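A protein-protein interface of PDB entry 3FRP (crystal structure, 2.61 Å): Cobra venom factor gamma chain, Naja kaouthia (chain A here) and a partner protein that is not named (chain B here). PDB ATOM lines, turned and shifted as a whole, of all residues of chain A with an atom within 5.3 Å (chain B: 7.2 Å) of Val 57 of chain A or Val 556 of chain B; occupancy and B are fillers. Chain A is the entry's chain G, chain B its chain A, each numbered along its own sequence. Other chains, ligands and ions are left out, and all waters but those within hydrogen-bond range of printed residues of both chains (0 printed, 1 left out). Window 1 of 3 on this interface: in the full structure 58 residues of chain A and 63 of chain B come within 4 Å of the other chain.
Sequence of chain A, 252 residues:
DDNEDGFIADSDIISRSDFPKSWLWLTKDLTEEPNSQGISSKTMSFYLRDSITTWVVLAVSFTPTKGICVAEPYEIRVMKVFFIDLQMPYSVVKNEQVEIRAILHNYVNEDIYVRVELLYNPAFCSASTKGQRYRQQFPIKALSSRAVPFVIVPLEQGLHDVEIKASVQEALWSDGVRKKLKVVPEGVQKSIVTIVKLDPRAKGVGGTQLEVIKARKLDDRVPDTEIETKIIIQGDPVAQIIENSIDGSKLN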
ATOM      1  N   SER A  22      -9.633   8.485 -23.085  1.00  0.00           N
ATOM      2  CA  SER A  22     -10.870   8.106 -22.410  1.00  0.00           C
ATOM      3  C   SER A  22     -10.676   6.824 -21.618  1.00  0.00           C
ATOM      4  O   SER A  22      -9.870   5.955 -21.996  1.00  0.00           O
ATOM      5  CB  SER A  22     -12.036   7.934 -23.402  1.00  0.00           C
ATOM      6  OG  SER A  22     -11.717   7.000 -24.420  1.00  0.00           O
ATOM      7  N   TRP A  23     -11.428   6.703 -20.526  1.00  0.00           N
ATOM      8  CA  TRP A  23     -11.319   5.548 -19.640  1.00  0.00           C
ATOM      9  C   TRP A  23     -12.536   5.526 -18.726  1.00  0.00           C
ATOM     10  O   TRP A  23     -13.479   6.290 -18.929  1.00  0.00           O
ATOM     11  CB  TRP A  23     -10.005   5.602 -18.837  1.00  0.00           C
ATOM     12  CG  TRP A  23      -9.820   6.897 -18.050  1.00  0.00           C
ATOM     13  CD1 TRP A  23      -9.551   8.145 -18.555  1.00  0.00           C
ATOM     14  CD2 TRP A  23      -9.882   7.050 -16.632  1.00  0.00           C
ATOM     15  NE1 TRP A  23      -9.461   9.057 -17.538  1.00  0.00           N
ATOM     16  CE2 TRP A  23      -9.653   8.410 -16.346  1.00  0.00           C
ATOM     17  CE3 TRP A  23     -10.118   6.170 -15.571  1.00  0.00           C
ATOM     18  CZ2 TRP A  23      -9.646   8.905 -15.042  1.00  0.00           C
ATOM     19  CZ3 TRP A  23     -10.117   6.663 -14.277  1.00  0.00           C
ATOM     20  CH2 TRP A  23      -9.877   8.015 -14.024  1.00  0.00           C
ATOM     21  N   LEU A  24     -12.493   4.670 -17.711  1.00  0.00           N
ATOM     22  CA  LEU A  24     -13.605   4.462 -16.787  1.00  0.00           C
ATOM     23  C   LEU A  24     -14.830   3.922 -17.514  1.00  0.00           C
ATOM     24  O   LEU A  24     -15.972   4.150 -17.101  1.00  0.00           O
ATOM     25  CB  LEU A  24     -13.948   5.737 -16.024  1.00  0.00           C
ATOM     26  CG  LEU A  24     -14.545   5.473 -14.646  1.00  0.00           C
ATOM     27  CD1 LEU A  24     -13.459   5.086 -13.662  1.00  0.00           C
ATOM     28  CD2 LEU A  24     -15.277   6.681 -14.163  1.00  0.00           C
ATOM     29  N   TRP A  25     -14.589   3.186 -18.599  1.00  0.00           N
ATOM     30  CA  TRP A  25     -15.675   2.579 -19.355  1.00  0.00           C
ATOM     31  C   TRP A  25     -16.247   1.409 -18.574  1.00  0.00           C
ATOM     32  O   TRP A  25     -15.951   0.260 -18.864  1.00  0.00           O
ATOM     33  CB  TRP A  25     -15.192   2.158 -20.740  1.00  0.00           C
ATOM     34  CG  TRP A  25     -16.295   1.776 -21.717  1.00  0.00           C
ATOM     35  CD1 TRP A  25     -16.513   0.538 -22.254  1.00  0.00           C
ATOM     36  CD2 TRP A  25     -17.314   2.641 -22.277  1.00  0.00           C
ATOM     37  NE1 TRP A  25     -17.588   0.580 -23.118  1.00  0.00           N
ATOM     38  CE2 TRP A  25     -18.099   1.854 -23.143  1.00  0.00           C
ATOM     39  CE3 TRP A  25     -17.633   4.000 -22.128  1.00  0.00           C
ATOM     40  CZ2 TRP A  25     -19.184   2.377 -23.856  1.00  0.00           C
ATOM     41  CZ3 TRP A  25     -18.710   4.521 -22.835  1.00  0.00           C
ATOM     42  CH2 TRP A  25     -19.476   3.706 -23.685  1.00  0.00           C
ATOM     43  N   TRP A  55     -11.090  16.208 -16.470  1.00  0.00           N
ATOM     44  CA  TRP A  55     -11.812  15.029 -16.899  1.00  0.00           C
ATOM     45  C   TRP A  55     -13.275  15.319 -16.733  1.00  0.00           C
ATOM     46  O   TRP A  55     -13.703  15.804 -15.696  1.00  0.00           O
ATOM     47  CB  TRP A  55     -11.494  13.818 -16.026  1.00  0.00           C
ATOM     48  CG  TRP A  55     -10.083  13.384 -16.026  1.00  0.00           C
ATOM     49  CD1 TRP A  55      -9.224  13.457 -14.987  1.00  0.00           C
ATOM     50  CD2 TRP A  55      -9.353  12.781 -17.113  1.00  0.00           C
ATOM     51  NE1 TRP A  55      -8.002  12.954 -15.342  1.00  0.00           N
ATOM     52  CE2 TRP A  55      -8.047  12.526 -16.640  1.00  0.00           C
ATOM     53  CE3 TRP A  55      -9.678  12.426 -18.435  1.00  0.00           C
ATOM     54  CZ2 TRP A  55      -7.059  11.947 -17.429  1.00  0.00           C
ATOM     55  CZ3 TRP A  55      -8.681  11.839 -19.232  1.00  0.00           C
ATOM     56  CH2 TRP A  55      -7.388  11.614 -18.722  1.00  0.00           C
ATOM     57  N   VAL A  56     -14.048  15.001 -17.754  1.00  0.00           N
ATOM     58  CA  VAL A  56     -15.489  15.023 -17.649  1.00  0.00           C
ATOM     59  C   VAL A  56     -15.961  13.574 -17.456  1.00  0.00           C
ATOM     60  O   VAL A  56     -15.590  12.687 -18.234  1.00  0.00           O
ATOM     61  CB  VAL A  56     -16.095  15.613 -18.924  1.00  0.00           C
ATOM     62  CG1 VAL A  56     -15.858  17.093 -18.988  1.00  0.00           C
ATOM     63  CG2 VAL A  56     -15.413  15.037 -20.070  1.00  0.00           C
ATOM     64  N   VAL A  57     -16.750  13.330 -16.415  1.00  0.00           N
ATOM     65  CA  VAL A  57     -17.340  12.015 -16.220  1.00  0.00           C
ATOM     66  C   VAL A  57     -18.829  12.043 -16.573  1.00  0.00           C
ATOM     67  O   VAL A  57     -19.606  12.802 -15.985  1.00  0.00           O
ATOM     68  CB  VAL A  57     -17.046  11.372 -14.794  1.00  0.00           C
ATOM     69  CG1 VAL A  57     -15.559  11.489 -14.421  1.00  0.00           C
ATOM     70  CG2 VAL A  57     -17.867  11.986 -13.718  1.00  0.00           C
ATOM     71  N   LEU A  58     -19.210  11.244 -17.574  1.00  0.00           N
ATOM     72  CA  LEU A  58     -20.615  11.172 -17.963  1.00  0.00           C
ATOM     73  C   LEU A  58     -21.243   9.862 -17.529  1.00  0.00           C
ATOM     74  O   LEU A  58     -20.726   8.797 -17.794  1.00  0.00           O
ATOM     75  CB  LEU A  58     -20.833  11.457 -19.464  1.00  0.00           C
ATOM     76  CG  LEU A  58     -22.317  11.541 -19.943  1.00  0.00           C
ATOM     77  CD1 LEU A  58     -23.238  12.420 -19.031  1.00  0.00           C
ATOM     78  CD2 LEU A  58     -22.492  11.968 -21.449  1.00  0.00           C
ATOM     79  N   ALA A  59     -22.362   9.962 -16.840  1.00  0.00           N
ATOM     80  CA  ALA A  59     -23.114   8.797 -16.434  1.00  0.00           C
ATOM     81  C   ALA A  59     -24.471   8.776 -17.120  1.00  0.00           C
ATOM     82  O   ALA A  59     -25.217   9.737 -17.040  1.00  0.00           O
ATOM     83  CB  ALA A  59     -23.277   8.770 -14.921  1.00  0.00           C
ATOM     84  N   GLU A  72     -25.996  15.121 -15.573  1.00  0.00           N
ATOM     85  CA  GLU A  72     -25.172  16.280 -15.872  1.00  0.00           C
ATOM     86  C   GLU A  72     -23.680  15.896 -15.780  1.00  0.00           C
ATOM     87  O   GLU A  72     -23.324  15.051 -14.955  1.00  0.00           O
ATOM     88  CB  GLU A  72     -25.530  17.404 -14.910  1.00  0.00           C
ATOM     89  CG  GLU A  72     -25.392  18.761 -15.521  1.00  0.00           C
ATOM     90  CD  GLU A  72     -26.562  19.151 -16.398  1.00  0.00           C
ATOM     91  OE1 GLU A  72     -27.022  20.297 -16.251  1.00  0.00           O
ATOM     92  OE2 GLU A  72     -27.024  18.340 -17.230  1.00  0.00           O
ATOM     93  N   PRO A  73     -22.803  16.504 -16.620  1.00  0.00           N
ATOM     94  CA  PRO A  73     -21.399  16.073 -16.565  1.00  0.00           C
ATOM     95  C   PRO A  73     -20.733  16.482 -15.251  1.00  0.00           C
ATOM     96  O   PRO A  73     -21.090  17.521 -14.678  1.00  0.00           O
ATOM     97  CB  PRO A  73     -20.746  16.814 -17.739  1.00  0.00           C
ATOM     98  CG  PRO A  73     -21.846  17.485 -18.490  1.00  0.00           C
ATOM     99  CD  PRO A  73     -22.988  17.637 -17.547  1.00  0.00           C
ATOM    100  N   TYR A  74     -19.786  15.682 -14.761  1.00  0.00           N
ATOM    101  CA  TYR A  74     -19.061  16.044 -13.541  1.00  0.00           C
ATOM    102  C   TYR A  74     -17.558  16.179 -13.804  1.00  0.00           C
ATOM    103  O   TYR A  74     -16.928  15.242 -14.310  1.00  0.00           O
ATOM    104  CB  TYR A  74     -19.336  15.060 -12.398  1.00  0.00           C
ATOM    105  CG  TYR A  74     -18.396  15.295 -11.247  1.00  0.00           C
ATOM    106  CD1 TYR A  74     -18.563  16.399 -10.405  1.00  0.00           C
ATOM    107  CD2 TYR A  74     -17.300  14.447 -11.026  1.00  0.00           C
ATOM    108  CE1 TYR A  74     -17.665  16.639  -9.360  1.00  0.00           C
ATOM    109  CE2 TYR A  74     -16.405  14.678  -9.984  1.00  0.00           C
ATOM    110  CZ  TYR A  74     -16.597  15.774  -9.158  1.00  0.00           C
ATOM    111  OH  TYR A  74     -15.728  16.011  -8.128  1.00  0.00           O
ATOM    112  N   GLU A  75     -16.989  17.338 -13.454  1.00  0.00           N
ATOM    113  CA  GLU A  75     -15.618  17.661 -13.850  1.00  0.00           C
ATOM    114  C   GLU A  75     -14.564  17.363 -12.781  1.00  0.00           C
ATOM    115  O   GLU A  75     -14.848  17.413 -11.589  1.00  0.00           O
ATOM    116  CB  GLU A  75     -15.524  19.114 -14.290  1.00  0.00           C
ATOM    117  CG  GLU A  75     -16.522  19.509 -15.356  1.00  0.00           C
ATOM    118  CD  GLU A  75     -15.989  20.596 -16.277  1.00  0.00           C
ATOM    119  OE1 GLU A  75     -15.307  21.512 -15.772  1.00  0.00           O
ATOM    120  OE2 GLU A  75     -16.246  20.537 -17.502  1.00  0.00           O
ATOM    121  N   ILE A  76     -13.351  17.045 -13.221  1.00  0.00           N
ATOM    122  CA  ILE A  76     -12.232  16.828 -12.319  1.00  0.00           C
ATOM    123  C   ILE A  76     -10.981  17.536 -12.837  1.00  0.00           C
ATOM    124  O   ILE A  76     -10.308  17.016 -13.744  1.00  0.00           O
ATOM    125  CB  ILE A  76     -11.897  15.315 -12.147  1.00  0.00           C
ATOM    126  CG1 ILE A  76     -13.110  14.531 -11.633  1.00  0.00           C
ATOM    127  CG2 ILE A  76     -10.654  15.125 -11.233  1.00  0.00           C
ATOM    128  CD1 ILE A  76     -12.890  13.025 -11.533  1.00  0.00           C
ATOM    129  N   GLN B 109     -24.715   5.575 -27.490  1.00  0.00           N
ATOM    130  CA  GLN B 109     -23.651   6.366 -26.897  1.00  0.00           C
ATOM    131  C   GLN B 109     -22.352   5.872 -27.446  1.00  0.00           C
ATOM    132  O   GLN B 109     -22.172   4.673 -27.576  1.00  0.00           O
ATOM    133  CB  GLN B 109     -23.634   6.210 -25.391  1.00  0.00           C
ATOM    134  CG  GLN B 109     -22.445   6.864 -24.720  1.00  0.00           C
ATOM    135  CD  GLN B 109     -22.463   6.665 -23.222  1.00  0.00           C
ATOM    136  OE1 GLN B 109     -22.984   5.665 -22.717  1.00  0.00           O
ATOM    137  NE2 GLN B 109     -21.900   7.618 -22.502  1.00  0.00           N
ATOM    138  N   THR B 110     -21.460   6.798 -27.791  1.00  0.00           N
ATOM    139  CA  THR B 110     -20.081   6.440 -28.065  1.00  0.00           C
ATOM    140  C   THR B 110     -19.133   7.079 -27.065  1.00  0.00           C
ATOM    141  O   THR B 110     -19.410   8.110 -26.450  1.00  0.00           O
ATOM    142  CB  THR B 110     -19.587   6.754 -29.512  1.00  0.00           C
ATOM    143  OG1 THR B 110     -19.411   8.162 -29.693  1.00  0.00           O
ATOM    144  CG2 THR B 110     -20.535   6.187 -30.573  1.00  0.00           C
ATOM    145  N   ASP B 111     -18.015   6.393 -26.932  1.00  0.00           N
ATOM    146  CA  ASP B 111     -16.849   6.767 -26.184  1.00  0.00           C
ATOM    147  C   ASP B 111     -16.460   8.242 -26.360  1.00  0.00           C
ATOM    148  O   ASP B 111     -16.375   9.012 -25.398  1.00  0.00           O
ATOM    149  CB  ASP B 111     -15.733   5.860 -26.710  1.00  0.00           C
ATOM    150  CG  ASP B 111     -14.471   6.071 -26.010  1.00  0.00           C
ATOM    151  OD1 ASP B 111     -13.450   6.286 -26.689  1.00  0.00           O
ATOM    152  OD2 ASP B 111     -14.524   6.049 -24.768  1.00  0.00           O
ATOM    153  N   LYS B 112     -16.210   8.609 -27.613  1.00  0.00           N
ATOM    154  CA  LYS B 112     -15.865   9.979 -27.995  1.00  0.00           C
ATOM    155  C   LYS B 112     -16.368  10.258 -29.407  1.00  0.00           C
ATOM    156  O   LYS B 112     -16.797   9.334 -30.112  1.00  0.00           O
ATOM    157  CB  LYS B 112     -14.353  10.207 -27.897  1.00  0.00           C
ATOM    158  CG  LYS B 112     -13.535   8.973 -28.141  1.00  0.00           C
ATOM    159  CD  LYS B 112     -12.066   9.182 -27.830  1.00  0.00           C
ATOM    160  CE  LYS B 112     -11.237   7.976 -28.273  1.00  0.00           C
ATOM    161  NZ  LYS B 112     -10.076   8.422 -29.125  1.00  0.00           N
ATOM    162  N   LEU B 122     -15.609   2.524 -28.367  1.00  0.00           N
ATOM    163  CA  LEU B 122     -16.441   1.917 -27.357  1.00  0.00           C
ATOM    164  C   LEU B 122     -17.815   2.523 -27.504  1.00  0.00           C
ATOM    165  O   LEU B 122     -17.953   3.735 -27.728  1.00  0.00           O
ATOM    166  CB  LEU B 122     -15.858   2.154 -25.970  1.00  0.00           C
ATOM    167  CG  LEU B 122     -14.443   1.569 -25.740  1.00  0.00           C
ATOM    168  CD1 LEU B 122     -13.671   2.348 -24.681  1.00  0.00           C
ATOM    169  CD2 LEU B 122     -14.537   0.108 -25.360  1.00  0.00           C
ATOM    170  N   ARG B 124     -22.308   1.917 -26.549  1.00  0.00           N
ATOM    171  CA  ARG B 124     -23.378   1.275 -25.842  1.00  0.00           C
ATOM    172  C   ARG B 124     -24.640   1.541 -26.638  1.00  0.00           C
ATOM    173  O   ARG B 124     -24.739   2.557 -27.334  1.00  0.00           O
ATOM    174  CB  ARG B 124     -23.500   1.850 -24.416  1.00  0.00           C
ATOM    175  CG  ARG B 124     -22.425   1.339 -23.457  1.00  0.00           C
ATOM    176  CD  ARG B 124     -22.748   1.590 -21.996  1.00  0.00           C
ATOM    177  NE  ARG B 124     -22.057   2.769 -21.503  1.00  0.00           N
ATOM    178  CZ  ARG B 124     -20.943   2.770 -20.773  1.00  0.00           C
ATOM    179  NH1 ARG B 124     -20.342   1.649 -20.401  1.00  0.00           N
ATOM    180  NH2 ARG B 124     -20.429   3.928 -20.404  1.00  0.00           N
ATOM    181  N   VAL B 528     -24.139  12.651 -10.547  1.00  0.00           N
ATOM    182  CA  VAL B 528     -22.783  12.249 -10.185  1.00  0.00           C
ATOM    183  C   VAL B 528     -22.192  13.316  -9.253  1.00  0.00           C
ATOM    184  O   VAL B 528     -21.811  14.408  -9.693  1.00  0.00           O
ATOM    185  CB  VAL B 528     -21.906  12.064 -11.442  1.00  0.00           C
ATOM    186  CG1 VAL B 528     -20.464  11.801 -11.060  1.00  0.00           C
ATOM    187  CG2 VAL B 528     -22.442  10.932 -12.293  1.00  0.00           C
ATOM    188  N   ILE B 543     -16.178   8.994  -6.057  1.00  0.00           N
ATOM    189  CA  ILE B 543     -17.384   9.684  -6.583  1.00  0.00           C
ATOM    190  C   ILE B 543     -18.681   9.005  -6.171  1.00  0.00           C
ATOM    191  O   ILE B 543     -18.699   7.812  -5.876  1.00  0.00           O
ATOM    192  CB  ILE B 543     -17.367   9.839  -8.107  1.00  0.00           C
ATOM    193  CG1 ILE B 543     -17.067   8.490  -8.760  1.00  0.00           C
ATOM    194  CG2 ILE B 543     -16.355  10.905  -8.516  1.00  0.00           C
ATOM    195  CD1 ILE B 543     -17.535   8.381 -10.157  1.00  0.00           C
ATOM    196  N   LEU B 545     -22.874   8.186  -6.863  1.00  0.00           N
ATOM    197  CA  LEU B 545     -23.899   8.017  -7.873  1.00  0.00           C
ATOM    198  C   LEU B 545     -25.235   7.916  -7.186  1.00  0.00           C
ATOM    199  O   LEU B 545     -25.469   6.984  -6.394  1.00  0.00           O
ATOM    200  CB  LEU B 545     -23.665   6.735  -8.654  1.00  0.00           C
ATOM    201  CG  LEU B 545     -22.447   6.656  -9.561  1.00  0.00           C
ATOM    202  CD1 LEU B 545     -22.506   5.338 -10.276  1.00  0.00           C
ATOM    203  CD2 LEU B 545     -22.419   7.799 -10.562  1.00  0.00           C
ATOM    204  N   GLY B 554     -24.156   3.613 -16.806  1.00  0.00           N
ATOM    205  CA  GLY B 554     -22.957   3.456 -17.614  1.00  0.00           C
ATOM    206  C   GLY B 554     -22.083   4.682 -17.533  1.00  0.00           C
ATOM    207  O   GLY B 554     -22.560   5.797 -17.727  1.00  0.00           O
ATOM    208  N   LEU B 555     -20.795   4.479 -17.266  1.00  0.00           N
ATOM    209  CA  LEU B 555     -19.917   5.597 -16.994  1.00  0.00           C
ATOM    210  C   LEU B 555     -18.816   5.721 -18.011  1.00  0.00           C
ATOM    211  O   LEU B 555     -18.442   4.753 -18.659  1.00  0.00           O
ATOM    212  CB  LEU B 555     -19.262   5.434 -15.627  1.00  0.00           C
ATOM    213  CG  LEU B 555     -20.072   5.269 -14.358  1.00  0.00           C
ATOM    214  CD1 LEU B 555     -19.224   4.519 -13.396  1.00  0.00           C
ATOM    215  CD2 LEU B 555     -20.430   6.622 -13.809  1.00  0.00           C
ATOM    216  N   VAL B 556     -18.269   6.918 -18.112  1.00  0.00           N
ATOM    217  CA  VAL B 556     -17.101   7.144 -18.935  1.00  0.00           C
ATOM    218  C   VAL B 556     -16.437   8.445 -18.470  1.00  0.00           C
ATOM    219  O   VAL B 556     -17.113   9.377 -18.025  1.00  0.00           O
ATOM    220  CB  VAL B 556     -17.469   7.211 -20.448  1.00  0.00           C
ATOM    221  CG1 VAL B 556     -18.458   8.323 -20.709  1.00  0.00           C
ATOM    222  CG2 VAL B 556     -16.214   7.369 -21.323  1.00  0.00           C
ATOM    223  N   ALA B 557     -15.119   8.478 -18.551  1.00  0.00           N
ATOM    224  CA  ALA B 557     -14.365   9.684 -18.323  1.00  0.00           C
ATOM    225  C   ALA B 557     -13.587  10.007 -19.589  1.00  0.00           C
ATOM    226  O   ALA B 557     -12.866   9.158 -20.130  1.00  0.00           O
ATOM    227  CB  ALA B 557     -13.426   9.519 -17.145  1.00  0.00           C
ATOM    228  N   VAL B 558     -13.755  11.244 -20.043  1.00  0.00           N
ATOM    229  CA  VAL B 558     -13.152  11.741 -21.269  1.00  0.00           C
ATOM    230  C   VAL B 558     -12.291  13.010 -20.986  1.00  0.00           C
ATOM    231  O   VAL B 558     -12.715  13.920 -20.265  1.00  0.00           O
ATOM    232  CB  VAL B 558     -14.258  12.086 -22.330  1.00  0.00           C
ATOM    233  CG1 VAL B 558     -13.626  12.483 -23.632  1.00  0.00           C
ATOM    234  CG2 VAL B 558     -15.169  10.922 -22.570  1.00  0.00           C
ATOM    235  N   TYR B 563     -13.869  17.186 -26.086  1.00  0.00           N
ATOM    236  CA  TYR B 563     -15.011  18.081 -26.395  1.00  0.00           C
ATOM    237  C   TYR B 563     -14.631  19.311 -27.243  1.00  0.00           C
ATOM    238  O   TYR B 563     -15.394  19.740 -28.124  1.00  0.00           O
ATOM    239  CB  TYR B 563     -15.639  18.591 -25.123  1.00  0.00           C
ATOM    240  CG  TYR B 563     -16.310  17.549 -24.310  1.00  0.00           C
ATOM    241  CD1 TYR B 563     -17.612  17.755 -23.841  1.00  0.00           C
ATOM    242  CD2 TYR B 563     -15.656  16.371 -23.975  1.00  0.00           C
ATOM    243  CE1 TYR B 563     -18.248  16.810 -23.070  1.00  0.00           C
ATOM    244  CE2 TYR B 563     -16.288  15.416 -23.223  1.00  0.00           C
ATOM    245  CZ  TYR B 563     -17.578  15.649 -22.776  1.00  0.00           C
ATOM    246  OH  TYR B 563     -18.205  14.717 -22.034  1.00  0.00           O
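O of Trp 23 of chain A lies within hydrogen-bond range of N of Ala 557 of chain B (2.8 Å).
O of Leu 24 of chain A sits close to O of Leu 555 of chain B (3.0 Å).
N of Val 558 of chain B lies within hydrogen-bond range of O of Val 56 of chain A (3.0 Å).
The backbone carbonyl oxygen (O) of Val 556 of chain B is in hydrogen-bond range of the backbone NH (N) of Leu 58 of chain A.
The side-chain carboxylate (OD1) of Asp 111 of chain B lies within hydrogen-bond range of the side-chain hydroxyl (OG) of Ser 22 of chain A, 2.9 Å away.
O of Tyr 74 of chain A is in hydrogen-bond range of N of Val 57 of chain A (2.8 Å).
The backbone carbonyl oxygen of Leu 555 of chain B sits at hydrogen-bond distance from the guanidinium group of Arg 124 of chain B, 2.8 Å away.
O of Trp 55 of chain A lies within hydrogen-bond range of N of Ile 76 of chain A (2.8 Å).
N of Arg 124 of chain B lies within hydrogen-bond range of O of Gln 109 of chain B (2.9 Å).
N of Asp 111 of chain B sits at hydrogen-bond distance from O of Leu 122 of chain B (2.8 Å).
Among the printed residues, pairs that only touch across the chains: Ser 22 of chain A with Ala 557 of chain B, Trp 23 of chain A with Val 556 of chain B, Leu 24 of chain A with Val 556 of chain B, Leu 24 of chain A with Ala 557 of chain B, Trp 25 of chain A with Leu 122 of chain B, Trp 25 of chain A with Arg 124 of chain B, Trp 25 of chain A with Leu 555 of chain B, Trp 25 of chain A with Val 556 of chain B, Trp 55 of chain A with Val 558 of chain B, Val 56 of chain A with Val 556 of chain B, Val 56 of chain A with Ala 557 of chain B, Val 56 of chain A with Tyr 563 of chain B, Val 57 of chain A with Val 528 of chain B, Val 57 of chain A with Val 556 of chain B, Val 57 of chain A with Ala 557 of chain B, Leu 58 of chain A with Gly 554 of chain B, Leu 58 of chain A with Leu 555 of chain B, Ala 59 of chain A with Val 528 of chain B, Ala 59 of chain A with Gly 554 of chain B, Ala 59 of chain A with Leu 555 of chain B and Tyr 74 of chain A with Val 528 of chain B.
Printed residues of chain B within 4 Å of Val 57 of chain A: Val 528, Val 556 and Ala 557.
Printed residues of chain B within 4 Å of Leu 58 of chain A: Gly 554, Leu 555 and Val 556.
Of the printed residues of chain A, Arg 124 of chain B touches Trp 25.
The nearest printed residue of chain B that does not touch Val 57 of chain A is Ile 543 of chain B (5.1 Å).
The nearest residue of chain A that does not touch Val 556 of chain B is Ser 22 of chain A (4.7 Å).
Of the 15 printed residues of chain B, 10 touch a printed residue of chain A.
Hydrophobic or aromatic side chains of chain B that line the printed part of chain A: Leu 122, Val 528, Leu 555, Val 556, Ala 557, Val 558 and Tyr 563.
Hydrophobic or aromatic side chains of chain A within 4 Å of the printed part of chain B: Trp 23, Leu 24, Trp 25, Trp 55, Val 56, Val 57, Ala 59 and Tyr 74.
Among the printed residues, 26 pairs touch across the chains.
Among the printed residues, no Asp or Glu carboxylate lies within 4 Å of a Lys or Arg side-chain nitrogen of the other chain.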
